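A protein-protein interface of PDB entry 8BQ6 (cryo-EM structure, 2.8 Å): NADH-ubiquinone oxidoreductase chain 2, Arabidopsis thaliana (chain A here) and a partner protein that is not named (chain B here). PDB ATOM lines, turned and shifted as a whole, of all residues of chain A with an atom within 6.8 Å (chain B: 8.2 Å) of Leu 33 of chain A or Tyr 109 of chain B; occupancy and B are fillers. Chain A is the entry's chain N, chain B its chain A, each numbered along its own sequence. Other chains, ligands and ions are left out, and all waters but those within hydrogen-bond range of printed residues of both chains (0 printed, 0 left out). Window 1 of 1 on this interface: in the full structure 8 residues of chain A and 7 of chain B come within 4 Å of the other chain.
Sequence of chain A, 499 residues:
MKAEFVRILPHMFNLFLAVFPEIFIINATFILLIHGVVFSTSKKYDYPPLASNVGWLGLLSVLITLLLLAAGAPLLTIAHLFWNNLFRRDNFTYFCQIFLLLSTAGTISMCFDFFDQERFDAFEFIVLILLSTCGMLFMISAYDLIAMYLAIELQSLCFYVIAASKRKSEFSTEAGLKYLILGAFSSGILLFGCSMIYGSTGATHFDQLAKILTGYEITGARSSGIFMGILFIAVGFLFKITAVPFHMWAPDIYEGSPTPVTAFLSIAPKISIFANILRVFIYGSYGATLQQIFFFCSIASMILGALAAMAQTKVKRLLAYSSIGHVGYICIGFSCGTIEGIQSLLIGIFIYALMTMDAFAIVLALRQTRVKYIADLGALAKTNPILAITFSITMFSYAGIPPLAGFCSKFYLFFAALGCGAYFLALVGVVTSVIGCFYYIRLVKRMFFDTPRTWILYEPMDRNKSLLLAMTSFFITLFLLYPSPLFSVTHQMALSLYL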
ATOM      1  N   ALA A  28       0.460  28.177  24.351  1.00  0.00           N
ATOM      2  CA  ALA A  28       1.311  27.268  23.595  1.00  0.00           C
ATOM      3  C   ALA A  28       0.817  25.831  23.711  1.00  0.00           C
ATOM      4  O   ALA A  28       0.872  25.067  22.739  1.00  0.00           O
ATOM      5  CB  ALA A  28       2.754  27.387  24.076  1.00  0.00           C
ATOM      6  N   THR A  29       0.338  25.443  24.896  1.00  0.00           N
ATOM      7  CA  THR A  29      -0.246  24.116  25.064  1.00  0.00           C
ATOM      8  C   THR A  29      -1.466  23.930  24.171  1.00  0.00           C
ATOM      9  O   THR A  29      -1.643  22.866  23.566  1.00  0.00           O
ATOM     10  CB  THR A  29      -0.610  23.893  26.532  1.00  0.00           C
ATOM     11  OG1 THR A  29       0.585  23.912  27.320  1.00  0.00           O
ATOM     12  CG2 THR A  29      -1.322  22.567  26.721  1.00  0.00           C
ATOM     13  N   PHE A  30      -2.317  24.953  24.074  1.00  0.00           N
ATOM     14  CA  PHE A  30      -3.460  24.857  23.166  1.00  0.00           C
ATOM     15  C   PHE A  30      -3.007  24.724  21.716  1.00  0.00           C
ATOM     16  O   PHE A  30      -3.554  23.911  20.956  1.00  0.00           O
ATOM     17  CB  PHE A  30      -4.376  26.070  23.323  1.00  0.00           C
ATOM     18  CG  PHE A  30      -5.034  26.163  24.665  1.00  0.00           C
ATOM     19  CD1 PHE A  30      -5.188  25.041  25.461  1.00  0.00           C
ATOM     20  CD2 PHE A  30      -5.502  27.377  25.131  1.00  0.00           C
ATOM     21  CE1 PHE A  30      -5.790  25.132  26.699  1.00  0.00           C
ATOM     22  CE2 PHE A  30      -6.106  27.471  26.369  1.00  0.00           C
ATOM     23  CZ  PHE A  30      -6.250  26.346  27.152  1.00  0.00           C
ATOM     24  N   ILE A  31      -2.011  25.517  21.315  1.00  0.00           N
ATOM     25  CA  ILE A  31      -1.504  25.442  19.947  1.00  0.00           C
ATOM     26  C   ILE A  31      -0.990  24.040  19.647  1.00  0.00           C
ATOM     27  O   ILE A  31      -1.275  23.472  18.585  1.00  0.00           O
ATOM     28  CB  ILE A  31      -0.418  26.511  19.717  1.00  0.00           C
ATOM     29  CG1 ILE A  31      -1.039  27.908  19.728  1.00  0.00           C
ATOM     30  CG2 ILE A  31       0.326  26.265  18.414  1.00  0.00           C
ATOM     31  CD1 ILE A  31      -0.031  29.019  19.829  1.00  0.00           C
ATOM     32  N   LEU A  32      -0.242  23.455  20.584  1.00  0.00           N
ATOM     33  CA  LEU A  32       0.282  22.109  20.382  1.00  0.00           C
ATOM     34  C   LEU A  32      -0.829  21.068  20.342  1.00  0.00           C
ATOM     35  O   LEU A  32      -0.764  20.124  19.551  1.00  0.00           O
ATOM     36  CB  LEU A  32       1.293  21.765  21.469  1.00  0.00           C
ATOM     37  CG  LEU A  32       2.573  22.583  21.368  1.00  0.00           C
ATOM     38  CD1 LEU A  32       3.443  22.394  22.599  1.00  0.00           C
ATOM     39  CD2 LEU A  32       3.301  22.208  20.103  1.00  0.00           C
ATOM     40  N   LEU A  33      -1.843  21.205  21.198  1.00  0.00           N
ATOM     41  CA  LEU A  33      -2.969  20.277  21.150  1.00  0.00           C
ATOM     42  C   LEU A  33      -3.619  20.292  19.774  1.00  0.00           C
ATOM     43  O   LEU A  33      -3.896  19.236  19.188  1.00  0.00           O
ATOM     44  CB  LEU A  33      -3.995  20.635  22.222  1.00  0.00           C
ATOM     45  CG  LEU A  33      -5.209  19.704  22.310  1.00  0.00           C
ATOM     46  CD1 LEU A  33      -4.809  18.261  22.604  1.00  0.00           C
ATOM     47  CD2 LEU A  33      -6.202  20.216  23.325  1.00  0.00           C
ATOM     48  N   ILE A  34      -3.854  21.487  19.237  1.00  0.00           N
ATOM     49  CA  ILE A  34      -4.507  21.589  17.936  1.00  0.00           C
ATOM     50  C   ILE A  34      -3.613  21.019  16.844  1.00  0.00           C
ATOM     51  O   ILE A  34      -4.068  20.259  15.984  1.00  0.00           O
ATOM     52  CB  ILE A  34      -4.895  23.045  17.643  1.00  0.00           C
ATOM     53  CG1 ILE A  34      -6.007  23.481  18.588  1.00  0.00           C
ATOM     54  CG2 ILE A  34      -5.362  23.181  16.214  1.00  0.00           C
ATOM     55  CD1 ILE A  34      -6.159  24.966  18.684  1.00  0.00           C
ATOM     56  N   HIS A  35      -2.330  21.382  16.863  1.00  0.00           N
ATOM     57  CA  HIS A  35      -1.397  20.916  15.844  1.00  0.00           C
ATOM     58  C   HIS A  35      -1.317  19.395  15.850  1.00  0.00           C
ATOM     59  O   HIS A  35      -1.392  18.740  14.800  1.00  0.00           O
ATOM     60  CB  HIS A  35      -0.027  21.549  16.103  1.00  0.00           C
ATOM     61  CG  HIS A  35       1.122  20.816  15.483  1.00  0.00           C
ATOM     62  ND1 HIS A  35       1.620  21.136  14.239  1.00  0.00           N
ATOM     63  CD2 HIS A  35       1.863  19.776  15.930  1.00  0.00           C
ATOM     64  CE1 HIS A  35       2.624  20.330  13.949  1.00  0.00           C
ATOM     65  NE2 HIS A  35       2.790  19.493  14.957  1.00  0.00           N
ATOM     66  N   GLY A  36      -1.205  18.816  17.046  1.00  0.00           N
ATOM     67  CA  GLY A  36      -1.132  17.375  17.154  1.00  0.00           C
ATOM     68  C   GLY A  36      -2.388  16.695  16.655  1.00  0.00           C
ATOM     69  O   GLY A  36      -2.320  15.745  15.874  1.00  0.00           O
ATOM     70  N   VAL A  37      -3.557  17.179  17.080  1.00  0.00           N
ATOM     71  CA  VAL A  37      -4.758  16.447  16.701  1.00  0.00           C
ATOM     72  C   VAL A  37      -5.058  16.635  15.218  1.00  0.00           C
ATOM     73  O   VAL A  37      -5.576  15.721  14.569  1.00  0.00           O
ATOM     74  CB  VAL A  37      -5.952  16.823  17.599  1.00  0.00           C
ATOM     75  CG1 VAL A  37      -6.636  18.104  17.144  1.00  0.00           C
ATOM     76  CG2 VAL A  37      -6.926  15.662  17.666  1.00  0.00           C
ATOM     77  N   VAL A  38      -4.707  17.789  14.645  1.00  0.00           N
ATOM     78  CA  VAL A  38      -4.934  18.003  13.220  1.00  0.00           C
ATOM     79  C   VAL A  38      -4.031  17.114  12.378  1.00  0.00           C
ATOM     80  O   VAL A  38      -4.490  16.480  11.421  1.00  0.00           O
ATOM     81  CB  VAL A  38      -4.762  19.489  12.866  1.00  0.00           C
ATOM     82  CG1 VAL A  38      -4.555  19.658  11.380  1.00  0.00           C
ATOM     83  CG2 VAL A  38      -5.998  20.257  13.281  1.00  0.00           C
ATOM     84  N   VAL A  54       5.828  17.116  18.806  1.00  0.00           N
ATOM     85  CA  VAL A  54       5.193  17.926  19.836  1.00  0.00           C
ATOM     86  C   VAL A  54       6.060  17.978  21.086  1.00  0.00           C
ATOM     87  O   VAL A  54       6.048  18.975  21.809  1.00  0.00           O
ATOM     88  CB  VAL A  54       3.767  17.396  20.110  1.00  0.00           C
ATOM     89  CG1 VAL A  54       3.177  18.004  21.368  1.00  0.00           C
ATOM     90  CG2 VAL A  54       2.862  17.712  18.925  1.00  0.00           C
ATOM     91  N   PHE A 123       0.806  12.091  21.330  1.00  0.00           N
ATOM     92  CA  PHE A 123       1.262  13.433  21.658  1.00  0.00           C
ATOM     93  C   PHE A 123       0.532  14.012  22.862  1.00  0.00           C
ATOM     94  O   PHE A 123       1.036  14.955  23.478  1.00  0.00           O
ATOM     95  CB  PHE A 123       1.095  14.355  20.452  1.00  0.00           C
ATOM     96  CG  PHE A 123      -0.326  14.752  20.198  1.00  0.00           C
ATOM     97  CD1 PHE A 123      -1.123  14.000  19.358  1.00  0.00           C
ATOM     98  CD2 PHE A 123      -0.871  15.863  20.811  1.00  0.00           C
ATOM     99  CE1 PHE A 123      -2.432  14.355  19.129  1.00  0.00           C
ATOM    100  CE2 PHE A 123      -2.178  16.213  20.589  1.00  0.00           C
ATOM    101  CZ  PHE A 123      -2.959  15.457  19.746  1.00  0.00           C
ATOM    102  N   GLU A 124      -0.653  13.488  23.192  1.00  0.00           N
ATOM    103  CA  GLU A 124      -1.397  13.976  24.348  1.00  0.00           C
ATOM    104  C   GLU A 124      -0.620  13.811  25.641  1.00  0.00           C
ATOM    105  O   GLU A 124      -0.920  14.491  26.625  1.00  0.00           O
ATOM    106  CB  GLU A 124      -2.737  13.258  24.458  1.00  0.00           C
ATOM    107  CG  GLU A 124      -3.683  13.542  23.313  1.00  0.00           C
ATOM    108  CD  GLU A 124      -3.549  12.578  22.150  1.00  0.00           C
ATOM    109  OE1 GLU A 124      -2.485  11.950  21.981  1.00  0.00           O
ATOM    110  OE2 GLU A 124      -4.532  12.440  21.400  1.00  0.00           O
ATOM    111  N   VAL A 127       0.995  17.101  26.028  1.00  0.00           N
ATOM    112  CA  VAL A 127      -0.014  18.091  26.393  1.00  0.00           C
ATOM    113  C   VAL A 127      -0.378  17.975  27.869  1.00  0.00           C
ATOM    114  O   VAL A 127      -0.504  18.984  28.570  1.00  0.00           O
ATOM    115  CB  VAL A 127      -1.249  17.957  25.483  1.00  0.00           C
ATOM    116  CG1 VAL A 127      -2.328  18.948  25.891  1.00  0.00           C
ATOM    117  CG2 VAL A 127      -0.852  18.189  24.036  1.00  0.00           C
ATOM    118  N   LEU A 131       0.072  20.734  30.796  1.00  0.00           N
ATOM    119  CA  LEU A 131      -1.048  21.197  31.611  1.00  0.00           C
ATOM    120  C   LEU A 131      -0.768  20.998  33.098  1.00  0.00           C
ATOM    121  O   LEU A 131      -1.107  21.859  33.921  1.00  0.00           O
ATOM    122  CB  LEU A 131      -2.339  20.490  31.199  1.00  0.00           C
ATOM    123  CG  LEU A 131      -2.916  20.846  29.827  1.00  0.00           C
ATOM    124  CD1 LEU A 131      -4.035  19.890  29.463  1.00  0.00           C
ATOM    125  CD2 LEU A 131      -3.410  22.279  29.800  1.00  0.00           C
ATOM    126  N   ILE B 102     -11.587  27.646  26.004  1.00  0.00           N
ATOM    127  CA  ILE B 102     -10.909  26.438  26.481  1.00  0.00           C
ATOM    128  C   ILE B 102     -11.787  25.205  26.259  1.00  0.00           C
ATOM    129  O   ILE B 102     -11.341  24.174  25.719  1.00  0.00           O
ATOM    130  CB  ILE B 102     -10.509  26.590  27.961  1.00  0.00           C
ATOM    131  CG1 ILE B 102      -9.397  27.629  28.115  1.00  0.00           C
ATOM    132  CG2 ILE B 102     -10.077  25.258  28.542  1.00  0.00           C
ATOM    133  CD1 ILE B 102      -9.583  28.561  29.279  1.00  0.00           C
ATOM    134  N   LEU B 103     -13.061  25.300  26.645  1.00  0.00           N
ATOM    135  CA  LEU B 103     -13.924  24.129  26.504  1.00  0.00           C
ATOM    136  C   LEU B 103     -14.204  23.796  25.036  1.00  0.00           C
ATOM    137  O   LEU B 103     -14.369  22.622  24.684  1.00  0.00           O
ATOM    138  CB  LEU B 103     -15.213  24.341  27.297  1.00  0.00           C
ATOM    139  CG  LEU B 103     -14.982  24.265  28.816  1.00  0.00           C
ATOM    140  CD1 LEU B 103     -16.238  23.920  29.571  1.00  0.00           C
ATOM    141  CD2 LEU B 103     -13.893  23.261  29.167  1.00  0.00           C
ATOM    142  N   THR B 104     -14.215  24.797  24.157  1.00  0.00           N
ATOM    143  CA  THR B 104     -14.419  24.553  22.735  1.00  0.00           C
ATOM    144  C   THR B 104     -13.183  23.953  22.077  1.00  0.00           C
ATOM    145  O   THR B 104     -13.306  23.193  21.113  1.00  0.00           O
ATOM    146  CB  THR B 104     -14.819  25.855  22.039  1.00  0.00           C
ATOM    147  OG1 THR B 104     -15.902  26.461  22.755  1.00  0.00           O
ATOM    148  CG2 THR B 104     -15.260  25.599  20.613  1.00  0.00           C
ATOM    149  N   ILE B 105     -11.989  24.275  22.578  1.00  0.00           N
ATOM    150  CA  ILE B 105     -10.802  23.551  22.134  1.00  0.00           C
ATOM    151  C   ILE B 105     -10.922  22.081  22.506  1.00  0.00           C
ATOM    152  O   ILE B 105     -10.588  21.189  21.712  1.00  0.00           O
ATOM    153  CB  ILE B 105      -9.532  24.181  22.727  1.00  0.00           C
ATOM    154  CG1 ILE B 105      -9.203  25.475  21.996  1.00  0.00           C
ATOM    155  CG2 ILE B 105      -8.355  23.225  22.621  1.00  0.00           C
ATOM    156  CD1 ILE B 105      -7.924  26.091  22.453  1.00  0.00           C
ATOM    157  N   GLY B 106     -11.406  21.805  23.718  1.00  0.00           N
ATOM    158  CA  GLY B 106     -11.702  20.421  24.066  1.00  0.00           C
ATOM    159  C   GLY B 106     -12.690  19.776  23.108  1.00  0.00           C
ATOM    160  O   GLY B 106     -12.513  18.627  22.690  1.00  0.00           O
ATOM    161  N   PHE B 107     -13.740  20.512  22.748  1.00  0.00           N
ATOM    162  CA  PHE B 107     -14.750  19.986  21.833  1.00  0.00           C
ATOM    163  C   PHE B 107     -14.160  19.680  20.458  1.00  0.00           C
ATOM    164  O   PHE B 107     -14.482  18.654  19.854  1.00  0.00           O
ATOM    165  CB  PHE B 107     -15.902  20.980  21.723  1.00  0.00           C
ATOM    166  CG  PHE B 107     -17.083  20.466  20.965  1.00  0.00           C
ATOM    167  CD1 PHE B 107     -17.743  19.323  21.371  1.00  0.00           C
ATOM    168  CD2 PHE B 107     -17.555  21.148  19.860  1.00  0.00           C
ATOM    169  CE1 PHE B 107     -18.836  18.863  20.672  1.00  0.00           C
ATOM    170  CE2 PHE B 107     -18.650  20.691  19.161  1.00  0.00           C
ATOM    171  CZ  PHE B 107     -19.291  19.553  19.568  1.00  0.00           C
ATOM    172  N   LEU B 108     -13.307  20.569  19.945  1.00  0.00           N
ATOM    173  CA  LEU B 108     -12.651  20.334  18.661  1.00  0.00           C
ATOM    174  C   LEU B 108     -11.729  19.123  18.722  1.00  0.00           C
ATOM    175  O   LEU B 108     -11.639  18.347  17.760  1.00  0.00           O
ATOM    176  CB  LEU B 108     -11.871  21.578  18.244  1.00  0.00           C
ATOM    177  CG  LEU B 108     -10.933  21.485  17.041  1.00  0.00           C
ATOM    178  CD1 LEU B 108     -11.704  21.138  15.782  1.00  0.00           C
ATOM    179  CD2 LEU B 108     -10.197  22.797  16.865  1.00  0.00           C
ATOM    180  N   TYR B 109     -11.026  18.951  19.840  1.00  0.00           N
ATOM    181  CA  TYR B 109     -10.239  17.738  20.011  1.00  0.00           C
ATOM    182  C   TYR B 109     -11.129  16.503  19.914  1.00  0.00           C
ATOM    183  O   TYR B 109     -10.820  15.556  19.184  1.00  0.00           O
ATOM    184  CB  TYR B 109      -9.498  17.771  21.346  1.00  0.00           C
ATOM    185  CG  TYR B 109      -8.748  16.500  21.631  1.00  0.00           C
ATOM    186  CD1 TYR B 109      -7.523  16.255  21.042  1.00  0.00           C
ATOM    187  CD2 TYR B 109      -9.267  15.541  22.481  1.00  0.00           C
ATOM    188  CE1 TYR B 109      -6.836  15.095  21.288  1.00  0.00           C
ATOM    189  CE2 TYR B 109      -8.586  14.379  22.735  1.00  0.00           C
ATOM    190  CZ  TYR B 109      -7.372  14.162  22.136  1.00  0.00           C
ATOM    191  OH  TYR B 109      -6.691  13.003  22.385  1.00  0.00           O
ATOM    192  N   GLU B 110     -12.261  16.517  20.623  1.00  0.00           N
ATOM    193  CA  GLU B 110     -13.167  15.371  20.598  1.00  0.00           C
ATOM    194  C   GLU B 110     -13.720  15.118  19.206  1.00  0.00           C
ATOM    195  O   GLU B 110     -13.901  13.968  18.795  1.00  0.00           O
ATOM    196  CB  GLU B 110     -14.317  15.591  21.565  1.00  0.00           C
ATOM    197  CG  GLU B 110     -14.155  14.870  22.850  1.00  0.00           C
ATOM    198  CD  GLU B 110     -14.660  15.693  23.984  1.00  0.00           C
ATOM    199  OE1 GLU B 110     -15.153  16.804  23.708  1.00  0.00           O
ATOM    200  OE2 GLU B 110     -14.587  15.228  25.138  1.00  0.00           O
ATOM    201  N   TRP B 111     -14.039  16.189  18.492  1.00  0.00           N
ATOM    202  CA  TRP B 111     -14.557  16.079  17.137  1.00  0.00           C
ATOM    203  C   TRP B 111     -13.546  15.418  16.212  1.00  0.00           C
ATOM    204  O   TRP B 111     -13.883  14.500  15.456  1.00  0.00           O
ATOM    205  CB  TRP B 111     -14.905  17.475  16.651  1.00  0.00           C
ATOM    206  CG  TRP B 111     -15.661  17.557  15.411  1.00  0.00           C
ATOM    207  CD1 TRP B 111     -15.376  16.952  14.230  1.00  0.00           C
ATOM    208  CD2 TRP B 111     -16.817  18.352  15.192  1.00  0.00           C
ATOM    209  NE1 TRP B 111     -16.300  17.305  13.286  1.00  0.00           N
ATOM    210  CE2 TRP B 111     -17.197  18.169  13.853  1.00  0.00           C
ATOM    211  CE3 TRP B 111     -17.575  19.198  16.000  1.00  0.00           C
ATOM    212  CZ2 TRP B 111     -18.300  18.796  13.305  1.00  0.00           C
ATOM    213  CZ3 TRP B 111     -18.667  19.819  15.455  1.00  0.00           C
ATOM    214  CH2 TRP B 111     -19.023  19.616  14.121  1.00  0.00           C
ATOM    215  N   LYS B 112     -12.297  15.883  16.253  1.00  0.00           N
ATOM    216  CA  LYS B 112     -11.291  15.365  15.333  1.00  0.00           C
ATOM    217  C   LYS B 112     -10.913  13.932  15.675  1.00  0.00           C
ATOM    218  O   LYS B 112     -10.385  13.202  14.830  1.00  0.00           O
ATOM    219  CB  LYS B 112     -10.058  16.260  15.357  1.00  0.00           C
ATOM    220  CG  LYS B 112     -10.256  17.598  14.691  1.00  0.00           C
ATOM    221  CD  LYS B 112     -10.685  17.442  13.255  1.00  0.00           C
ATOM    222  CE  LYS B 112      -9.481  17.338  12.341  1.00  0.00           C
ATOM    223  NZ  LYS B 112      -9.707  16.336  11.270  1.00  0.00           N
ATOM    224  N   ARG B 113     -11.175  13.512  16.905  1.00  0.00           N
ATOM    225  CA  ARG B 113     -10.833  12.162  17.311  1.00  0.00           C
ATOM    226  C   ARG B 113     -11.949  11.162  17.062  1.00  0.00           C
ATOM    227  O   ARG B 113     -11.797   9.991  17.421  1.00  0.00           O
ATOM    228  CB  ARG B 113     -10.452  12.148  18.785  1.00  0.00           C
ATOM    229  CG  ARG B 113      -9.029  12.551  19.033  1.00  0.00           C
ATOM    230  CD  ARG B 113      -8.148  11.352  18.831  1.00  0.00           C
ATOM    231  NE  ARG B 113      -6.751  11.636  19.120  1.00  0.00           N
ATOM    232  CZ  ARG B 113      -5.798  11.793  18.212  1.00  0.00           C
ATOM    233  NH1 ARG B 113      -6.055  11.723  16.916  1.00  0.00           N
ATOM    234  NH2 ARG B 113      -4.551  12.007  18.617  1.00  0.00           N
ATOM    235  N   GLY B 114     -13.057  11.589  16.467  1.00  0.00           N
ATOM    236  CA  GLY B 114     -14.150  10.688  16.173  1.00  0.00           C
ATOM    237  C   GLY B 114     -15.002  10.285  17.354  1.00  0.00           C
ATOM    238  O   GLY B 114     -15.619   9.215  17.312  1.00  0.00           O
ATOM    239  N   ALA B 115     -15.049  11.097  18.409  1.00  0.00           N
ATOM    240  CA  ALA B 115     -15.947  10.817  19.522  1.00  0.00           C
ATOM    241  C   ALA B 115     -17.379  11.237  19.226  1.00  0.00           C
ATOM    242  O   ALA B 115     -18.294  10.813  19.936  1.00  0.00           O
ATOM    243  CB  ALA B 115     -15.457  11.519  20.786  1.00  0.00           C
ATOM    244  N   LEU B 116     -17.584  12.055  18.197  1.00  0.00           N
ATOM    245  CA  LEU B 116     -18.901  12.518  17.787  1.00  0.00           C
ATOM    246  C   LEU B 116     -19.483  11.685  16.650  1.00  0.00           C
ATOM    247  O   LEU B 116     -20.518  12.058  16.090  1.00  0.00           O
ATOM    248  CB  LEU B 116     -18.828  13.992  17.380  1.00  0.00           C
ATOM    249  CG  LEU B 116     -18.288  14.966  18.428  1.00  0.00           C
ATOM    250  CD1 LEU B 116     -18.516  16.393  18.003  1.00  0.00           C
ATOM    251  CD2 LEU B 116     -18.981  14.710  19.738  1.00  0.00           C
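The side-chain carboxylate (OE2) of Glu 124 of chain A lies within hydrogen-bond range of the side-chain hydroxyl (OH) of Tyr 109 of chain B.
OE2 of Glu 124 of chain A is in salt-bridge range of NH2 of Arg 113 of chain B (2.8 Å).
Ile 102 of chain B touches Phe 30 of chain A (CG1 to CZ, 3.5 Å).
CG of Phe 30 of chain A touches CD1 of Ile 105 of chain B, at 3.6 Å.
Leu 33 of chain A touches Ile 105 of chain B (CD2 to CG2, 3.8 Å).
Leu 33 of chain A touches Tyr 109 of chain B.
CG2 of Val 37 of chain A touches CD1 of Tyr 109 of chain B, at 3.5 Å.
Lys 112 of chain B touches Val 37 of chain A (CB to CG2, 3.9 Å).
Arg 113 of chain B touches Val 37 of chain A (CG to CG2, 3.996 Å).
CE1 of Phe 123 of chain A touches NH2 of Arg 113 of chain B, 3.2 Å away.
Of the printed residues of chain B, Phe 30 of chain A touches Ile 102 (3.5 Å) and Ile 105 (3.6 Å).
Of the printed residues of chain B, Val 37 of chain A touches Tyr 109, Lys 112 and Arg 113.
Of the printed residues of chain B, Phe 123 of chain A touches Arg 113.
Of the printed residues of chain A, Ile 105 of chain B touches Phe 30 and Leu 33.
The nearest residue of chain B that does not touch Leu 33 of chain A is Gly 106 of chain B (5.5 Å).
The nearest printed residue of chain A that does not touch Arg 113 of chain B is Gly 36 of chain A (5.1 Å).
Of the 15 printed residues of chain B, 5 touch a printed residue of chain A.
Printed residues of chain B that touch a printed residue of chain A: Ile 102, Ile 105, Tyr 109, Lys 112 and Arg 113.
Of the 16 printed residues of chain A, 5 touch a printed residue of chain B.
Printed residues of chain A that touch a printed residue of chain B: Phe 30, Leu 33, Val 37, Phe 123 and Glu 124.
Hydrophobic or aromatic side chains of chain A that line the printed part of chain B: Phe 30, Leu 33, Val 37 and Phe 123.
Among the printed residues, 10 pairs touch across the chains.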
